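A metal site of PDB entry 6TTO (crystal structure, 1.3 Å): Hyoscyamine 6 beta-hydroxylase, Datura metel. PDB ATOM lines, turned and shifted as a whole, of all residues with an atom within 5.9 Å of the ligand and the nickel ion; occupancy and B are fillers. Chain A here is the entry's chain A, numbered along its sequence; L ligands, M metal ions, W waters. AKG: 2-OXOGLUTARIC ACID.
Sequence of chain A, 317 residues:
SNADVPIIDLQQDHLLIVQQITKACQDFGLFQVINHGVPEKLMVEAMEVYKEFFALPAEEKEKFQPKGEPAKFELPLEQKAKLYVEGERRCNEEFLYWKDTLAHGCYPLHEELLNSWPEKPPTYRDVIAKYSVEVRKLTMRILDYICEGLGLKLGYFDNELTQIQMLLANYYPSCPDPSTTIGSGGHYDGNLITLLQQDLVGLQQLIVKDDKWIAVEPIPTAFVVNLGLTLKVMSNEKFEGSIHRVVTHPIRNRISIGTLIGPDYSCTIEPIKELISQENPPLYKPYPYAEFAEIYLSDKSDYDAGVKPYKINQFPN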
ATOM      1  N   LYS A  99      24.785 -18.883   8.539  1.00  0.00           N
ATOM      2  CA  LYS A  99      24.493 -19.060   7.126  1.00  0.00           C
ATOM      3  C   LYS A  99      23.046 -19.509   7.009  1.00  0.00           C
ATOM      4  O   LYS A  99      22.663 -20.509   7.616  1.00  0.00           O
ATOM      5  CB  LYS A  99      25.408 -20.135   6.548  1.00  0.00           C
ATOM      6  CG  LYS A  99      25.107 -20.546   5.119  1.00  0.00           C
ATOM      7  CD  LYS A  99      25.805 -21.852   4.790  1.00  0.00           C
ATOM      8  CE  LYS A  99      25.346 -22.361   3.432  1.00  0.00           C
ATOM      9  NZ  LYS A  99      25.433 -23.829   3.274  1.00  0.00           N
ATOM     10  N   LEU A 168      18.775 -24.479  -3.566  1.00  0.00           N
ATOM     11  CA  LEU A 168      19.319 -23.954  -2.302  1.00  0.00           C
ATOM     12  C   LEU A 168      19.750 -22.520  -2.545  1.00  0.00           C
ATOM     13  O   LEU A 168      20.719 -22.292  -3.286  1.00  0.00           O
ATOM     14  CB  LEU A 168      20.494 -24.761  -1.825  1.00  0.00           C
ATOM     15  CG  LEU A 168      20.182 -26.019  -0.988  1.00  0.00           C
ATOM     16  CD1 LEU A 168      19.382 -27.050  -1.733  1.00  0.00           C
ATOM     17  CD2 LEU A 168      21.476 -26.590  -0.446  1.00  0.00           C
ATOM     18  N   ASN A 170      21.381 -19.557  -0.822  1.00  0.00           N
ATOM     19  CA  ASN A 170      22.192 -19.304   0.367  1.00  0.00           C
ATOM     20  C   ASN A 170      22.356 -17.827   0.587  1.00  0.00           C
ATOM     21  O   ASN A 170      22.449 -17.020  -0.359  1.00  0.00           O
ATOM     22  CB  ASN A 170      23.552 -19.955   0.174  1.00  0.00           C
ATOM     23  CG  ASN A 170      23.424 -21.384  -0.231  1.00  0.00           C
ATOM     24  OD1 ASN A 170      22.887 -22.207   0.507  1.00  0.00           O
ATOM     25  ND2 ASN A 170      23.859 -21.678  -1.441  1.00  0.00           N
ATOM     26  N   TYR A 172      24.803 -15.361   2.998  1.00  0.00           N
ATOM     27  CA  TYR A 172      25.986 -15.288   3.833  1.00  0.00           C
ATOM     28  C   TYR A 172      26.105 -13.867   4.358  1.00  0.00           C
ATOM     29  O   TYR A 172      26.525 -12.964   3.616  1.00  0.00           O
ATOM     30  CB  TYR A 172      27.244 -15.665   3.027  1.00  0.00           C
ATOM     31  CG  TYR A 172      27.184 -17.025   2.361  1.00  0.00           C
ATOM     32  CD1 TYR A 172      26.682 -17.163   1.064  1.00  0.00           C
ATOM     33  CD2 TYR A 172      27.679 -18.144   2.982  1.00  0.00           C
ATOM     34  CE1 TYR A 172      26.648 -18.404   0.448  1.00  0.00           C
ATOM     35  CE2 TYR A 172      27.638 -19.378   2.366  1.00  0.00           C
ATOM     36  CZ  TYR A 172      27.161 -19.503   1.102  1.00  0.00           C
ATOM     37  OH  TYR A 172      27.132 -20.783   0.544  1.00  0.00           O
ATOM     38  N   SER A 184      30.853 -21.226   4.740  1.00  0.00           N
ATOM     39  CA  SER A 184      30.474 -22.601   4.409  1.00  0.00           C
ATOM     40  C   SER A 184      31.747 -23.435   4.248  1.00  0.00           C
ATOM     41  O   SER A 184      32.533 -23.218   3.321  1.00  0.00           O
ATOM     42  CB  SER A 184      29.646 -22.621   3.123  1.00  0.00           C
ATOM     43  OG  SER A 184      29.122 -23.917   2.876  1.00  0.00           O
ATOM     44  N   HIS A 187      33.565 -28.883   1.217  1.00  0.00           N
ATOM     45  CA  HIS A 187      32.767 -30.090   1.044  1.00  0.00           C
ATOM     46  C   HIS A 187      32.767 -30.469  -0.429  1.00  0.00           C
ATOM     47  O   HIS A 187      32.982 -29.631  -1.312  1.00  0.00           O
ATOM     48  CB  HIS A 187      31.309 -29.899   1.470  1.00  0.00           C
ATOM     49  CG  HIS A 187      30.595 -28.831   0.696  1.00  0.00           C
ATOM     50  ND1 HIS A 187      30.791 -27.481   0.931  1.00  0.00           N
ATOM     51  CD2 HIS A 187      29.727 -28.904  -0.344  1.00  0.00           C
ATOM     52  CE1 HIS A 187      30.065 -26.784   0.072  1.00  0.00           C
ATOM     53  NE2 HIS A 187      29.378 -27.617  -0.682  1.00  0.00           N
ATOM     54  N   TYR A 188      32.513 -31.750  -0.684  1.00  0.00           N
ATOM     55  CA  TYR A 188      31.913 -32.158  -1.935  1.00  0.00           C
ATOM     56  C   TYR A 188      30.408 -31.995  -1.786  1.00  0.00           C
ATOM     57  O   TYR A 188      29.884 -32.202  -0.686  1.00  0.00           O
ATOM     58  CB  TYR A 188      32.081 -33.644  -2.209  1.00  0.00           C
ATOM     59  CG  TYR A 188      33.445 -34.188  -2.505  1.00  0.00           C
ATOM     60  CD1 TYR A 188      33.972 -34.147  -3.797  1.00  0.00           C
ATOM     61  CD2 TYR A 188      34.175 -34.878  -1.525  1.00  0.00           C
ATOM     62  CE1 TYR A 188      35.194 -34.728  -4.076  1.00  0.00           C
ATOM     63  CE2 TYR A 188      35.396 -35.446  -1.794  1.00  0.00           C
ATOM     64  CZ  TYR A 188      35.892 -35.393  -3.067  1.00  0.00           C
ATOM     65  OH  TYR A 188      37.094 -35.981  -3.359  1.00  0.00           O
ATOM     66  N   ASP A 189      29.712 -31.688  -2.869  1.00  0.00           N
ATOM     67  CA  ASP A 189      28.275 -31.885  -2.909  1.00  0.00           C
ATOM     68  C   ASP A 189      28.017 -33.390  -2.997  1.00  0.00           C
ATOM     69  O   ASP A 189      28.797 -34.123  -3.595  1.00  0.00           O
ATOM     70  CB  ASP A 189      27.649 -31.176  -4.120  1.00  0.00           C
ATOM     71  CG  ASP A 189      27.662 -29.659  -3.991  1.00  0.00           C
ATOM     72  OD1 ASP A 189      28.119 -29.131  -2.964  1.00  0.00           O
ATOM     73  OD2 ASP A 189      27.171 -28.988  -4.932  1.00  0.00           O
ATOM     74  N   THR A 194      25.679 -30.107  -9.702  1.00  0.00           N
ATOM     75  CA  THR A 194      25.131 -28.868  -9.173  1.00  0.00           C
ATOM     76  C   THR A 194      25.473 -27.729 -10.127  1.00  0.00           C
ATOM     77  O   THR A 194      26.595 -27.637 -10.593  1.00  0.00           O
ATOM     78  CB  THR A 194      25.748 -28.587  -7.798  1.00  0.00           C
ATOM     79  OG1 THR A 194      25.345 -29.633  -6.923  1.00  0.00           O
ATOM     80  CG2 THR A 194      25.265 -27.262  -7.248  1.00  0.00           C
ATOM     81  N   LEU A 196      25.451 -23.531 -10.017  1.00  0.00           N
ATOM     82  CA  LEU A 196      25.481 -22.477  -9.011  1.00  0.00           C
ATOM     83  C   LEU A 196      25.592 -21.124  -9.699  1.00  0.00           C
ATOM     84  O   LEU A 196      26.491 -20.900 -10.536  1.00  0.00           O
ATOM     85  CB  LEU A 196      26.672 -22.735  -8.086  1.00  0.00           C
ATOM     86  CG  LEU A 196      26.949 -21.939  -6.836  1.00  0.00           C
ATOM     87  CD1 LEU A 196      27.469 -20.574  -7.157  1.00  0.00           C
ATOM     88  CD2 LEU A 196      25.782 -21.906  -5.903  1.00  0.00           C
ATOM     89  N   GLN A 198      26.221 -17.148  -9.017  1.00  0.00           N
ATOM     90  CA  GLN A 198      26.801 -16.234  -8.046  1.00  0.00           C
ATOM     91  C   GLN A 198      27.140 -14.912  -8.737  1.00  0.00           C
ATOM     92  O   GLN A 198      27.348 -14.863  -9.953  1.00  0.00           O
ATOM     93  CB  GLN A 198      28.079 -16.804  -7.405  1.00  0.00           C
ATOM     94  CG  GLN A 198      29.115 -17.193  -8.442  1.00  0.00           C
ATOM     95  CD  GLN A 198      30.512 -17.397  -7.888  1.00  0.00           C
ATOM     96  OE1 GLN A 198      30.765 -17.267  -6.663  1.00  0.00           O
ATOM     97  NE2 GLN A 198      31.441 -17.751  -8.760  1.00  0.00           N
ATOM     98  N   LEU A 203      33.433 -17.926  -3.421  1.00  0.00           N
ATOM     99  CA  LEU A 203      33.523 -19.349  -3.727  1.00  0.00           C
ATOM    100  C   LEU A 203      34.968 -19.717  -4.065  1.00  0.00           C
ATOM    101  O   LEU A 203      35.617 -19.039  -4.873  1.00  0.00           O
ATOM    102  CB  LEU A 203      32.585 -19.725  -4.864  1.00  0.00           C
ATOM    103  CG  LEU A 203      32.535 -21.201  -5.245  1.00  0.00           C
ATOM    104  CD1 LEU A 203      31.984 -22.076  -4.141  1.00  0.00           C
ATOM    105  CD2 LEU A 203      31.682 -21.323  -6.509  1.00  0.00           C
ATOM    106  N   ASN A 226      29.497 -27.990 -10.781  1.00  0.00           N
ATOM    107  CA  ASN A 226      30.384 -28.823  -9.998  1.00  0.00           C
ATOM    108  C   ASN A 226      29.807 -30.210  -9.823  1.00  0.00           C
ATOM    109  O   ASN A 226      28.615 -30.399  -9.571  1.00  0.00           O
ATOM    110  CB  ASN A 226      30.763 -28.196  -8.680  1.00  0.00           C
ATOM    111  CG  ASN A 226      29.614 -28.083  -7.751  1.00  0.00           C
ATOM    112  OD1 ASN A 226      28.852 -27.124  -7.821  1.00  0.00           O
ATOM    113  ND2 ASN A 226      29.469 -29.052  -6.870  1.00  0.00           N
ATOM    114  N   HIS A 244      34.795 -27.670  -2.555  1.00  0.00           N
ATOM    115  CA  HIS A 244      34.671 -26.218  -2.621  1.00  0.00           C
ATOM    116  C   HIS A 244      34.221 -25.699  -1.267  1.00  0.00           C
ATOM    117  O   HIS A 244      33.729 -26.456  -0.421  1.00  0.00           O
ATOM    118  CB  HIS A 244      33.734 -25.791  -3.776  1.00  0.00           C
ATOM    119  CG  HIS A 244      32.404 -26.478  -3.728  1.00  0.00           C
ATOM    120  ND1 HIS A 244      32.171 -27.713  -4.260  1.00  0.00           N
ATOM    121  CD2 HIS A 244      31.224 -26.081  -3.176  1.00  0.00           C
ATOM    122  CE1 HIS A 244      30.918 -28.058  -4.043  1.00  0.00           C
ATOM    123  NE2 HIS A 244      30.327 -27.102  -3.356  1.00  0.00           N
ATOM    124  N   ARG A 245      34.400 -24.397  -1.067  1.00  0.00           N
ATOM    125  CA  ARG A 245      34.017 -23.747   0.180  1.00  0.00           C
ATOM    126  C   ARG A 245      33.644 -22.307  -0.129  1.00  0.00           C
ATOM    127  O   ARG A 245      33.939 -21.787  -1.207  1.00  0.00           O
ATOM    128  CB  ARG A 245      35.159 -23.774   1.217  1.00  0.00           C
ATOM    129  CG  ARG A 245      36.314 -22.810   0.901  1.00  0.00           C
ATOM    130  CD  ARG A 245      37.476 -22.965   1.861  1.00  0.00           C
ATOM    131  NE  ARG A 245      38.538 -22.014   1.557  1.00  0.00           N
ATOM    132  CZ  ARG A 245      39.687 -21.939   2.219  1.00  0.00           C
ATOM    133  NH1 ARG A 245      39.922 -22.755   3.231  1.00  0.00           N
ATOM    134  NH2 ARG A 245      40.607 -21.041   1.860  1.00  0.00           N
ATOM    135  N   VAL A 246      33.048 -21.645   0.851  1.00  0.00           N
ATOM    136  CA  VAL A 246      32.681 -20.223   0.732  1.00  0.00           C
ATOM    137  C   VAL A 246      33.309 -19.416   1.861  1.00  0.00           C
ATOM    138  O   VAL A 246      33.177 -19.785   3.033  1.00  0.00           O
ATOM    139  CB  VAL A 246      31.175 -20.007   0.703  1.00  0.00           C
ATOM    140  CG1 VAL A 246      30.828 -18.503   0.642  1.00  0.00           C
ATOM    141  CG2 VAL A 246      30.561 -20.725  -0.479  1.00  0.00           C
ATOM    142  N   ARG A 254      26.324 -11.934   0.741  1.00  0.00           N
ATOM    143  CA  ARG A 254      26.399 -12.655  -0.517  1.00  0.00           C
ATOM    144  C   ARG A 254      25.244 -13.629  -0.624  1.00  0.00           C
ATOM    145  O   ARG A 254      24.925 -14.327   0.330  1.00  0.00           O
ATOM    146  CB  ARG A 254      27.703 -13.437  -0.571  1.00  0.00           C
ATOM    147  CG  ARG A 254      27.906 -14.242  -1.864  1.00  0.00           C
ATOM    148  CD  ARG A 254      29.315 -14.820  -1.917  1.00  0.00           C
ATOM    149  NE  ARG A 254      29.531 -15.711  -3.073  1.00  0.00           N
ATOM    150  CZ  ARG A 254      29.145 -16.983  -3.117  1.00  0.00           C
ATOM    151  NH1 ARG A 254      28.548 -17.524  -2.065  1.00  0.00           N
ATOM    152  NH2 ARG A 254      29.341 -17.701  -4.213  1.00  0.00           N
ATOM    153  N   SER A 256      23.899 -16.834  -3.154  1.00  0.00           N
ATOM    154  CA  SER A 256      24.100 -17.726  -4.301  1.00  0.00           C
ATOM    155  C   SER A 256      22.876 -18.599  -4.478  1.00  0.00           C
ATOM    156  O   SER A 256      22.120 -18.858  -3.541  1.00  0.00           O
ATOM    157  CB  SER A 256      25.331 -18.583  -4.116  1.00  0.00           C
ATOM    158  OG  SER A 256      25.147 -19.426  -2.999  1.00  0.00           O
ATOM    159  N   LEU A 260      20.749 -28.344  -7.195  1.00  0.00           N
ATOM    160  CA  LEU A 260      21.421 -29.573  -6.848  1.00  0.00           C
ATOM    161  C   LEU A 260      20.572 -30.741  -7.345  1.00  0.00           C
ATOM    162  O   LEU A 260      19.499 -31.029  -6.778  1.00  0.00           O
ATOM    163  CB  LEU A 260      21.603 -29.677  -5.332  1.00  0.00           C
ATOM    164  CG  LEU A 260      22.711 -28.815  -4.703  1.00  0.00           C
ATOM    165  CD1 LEU A 260      22.418 -27.357  -4.783  1.00  0.00           C
ATOM    166  CD2 LEU A 260      22.949 -29.261  -3.244  1.00  0.00           C
HETATM  167  C1  AKG L   1      26.335 -25.650  -1.617  1.00  0.00           C
HETATM  168  O1  AKG L   1      26.567 -26.882  -1.688  1.00  0.00           O
HETATM  169  O2  AKG L   1      25.217 -25.203  -1.247  1.00  0.00           O
HETATM  170  C2  AKG L   1      27.427 -24.683  -2.028  1.00  0.00           C
HETATM  171  O5  AKG L   1      28.540 -25.113  -2.196  1.00  0.00           O
HETATM  172  C3  AKG L   1      27.097 -23.192  -2.209  1.00  0.00           C
HETATM  173  C4  AKG L   1      28.318 -22.473  -2.747  1.00  0.00           C
HETATM  174  C5  AKG L   1      28.126 -20.964  -2.876  1.00  0.00           C
HETATM  175  O3  AKG L   1      28.663 -20.397  -3.820  1.00  0.00           O
HETATM  176  O4  AKG L   1      27.451 -20.303  -2.063  1.00  0.00           O
HETATM  177 NI    NI M   1      28.451 -27.164  -2.477  1.00  0.00          NI
HETATM  178  O   HOH W   1      27.560 -26.599  -4.343  1.00  0.00           O
HETATM  179  O   HOH W   2      24.661 -27.078   1.120  1.00  0.00           O
HETATM  180  O   HOH W   3      25.443 -29.206  -0.674  1.00  0.00           O
HETATM  181  O   HOH W   4      23.949 -24.490   1.018  1.00  0.00           O
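OG of Ser 256 sits at hydrogen-bond distance from O4 of the ligand.
The side-chain hydroxyl (OH) of Tyr 172 lies within hydrogen-bond range of an oxygen (O4) of the ligand.
NH2 of Arg 254 is in salt-bridge range of O3 of the ligand, at 2.8 Å.
OD2 of Asp 189 sits at hydrogen-bond distance from OG1 of Thr 194.
The side-chain amide nitrogen (ND2) of Asn 226 is in hydrogen-bond range of the side-chain carboxylate (OD2) of Asp 189, at 3.0 Å.
The backbone NH (N) of Tyr 172 sits at hydrogen-bond distance from the backbone carbonyl oxygen (O) of Arg 254 (2.9 Å).
The guanidinium group (NH2) of Arg 254 lies within hydrogen-bond range of the side-chain amide oxygen (OE1) of Gln 198, at 2.9 Å.
The backbone carbonyl oxygen of Ser 184 sits at hydrogen-bond distance from the backbone NH of Val 246 (3.0 Å).
The backbone carbonyl oxygen of Ser 256 sits at hydrogen-bond distance from the backbone NH of Asn 170, 2.9 Å away.
ND2 of Asn 170 touches C3 of the ligand (3.7 Å).
Leu 196 touches the ligand (CD1 to O3, 3.5 Å).
Leu 203 touches the ligand (CD1 to O3, 3.7 Å).
CG2 of Val 246 touches C5 of the ligand, 3.4 Å away.
Within 4 Å of the ligand: Asn 170, Tyr 172, His 187, Asp 189, Leu 196, Leu 203, His 244, Val 246, Arg 254 and Ser 256.
The nearest printed residue that does not touch the ligand is Leu 168 (4.1 Å).
Of the 19 residues printed, 3 come within 4 Å of the nickel ion.
The nickel ion is bound by OD1 of Asp 189 (2.1 Å).
O1 of the ligand binds the nickel ion (2.1 Å).
The nickel ion is bound by a ring nitrogen (NE2) of His 187, at 2.1 Å.
NE2 of His 244 is bound to the nickel ion.
The nickel ion is bound by O5 of the ligand.
The nickel ion is bound by water W1, at 2.1 Å.
The nickel ion has six donor atoms within binding distance.
Water W4 lies within hydrogen-bond range of the side-chain amide oxygen (OD1) of Asn 170, an oxygen (O2) of the ligand and the side-chain amino group (NZ) of Lys 99.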
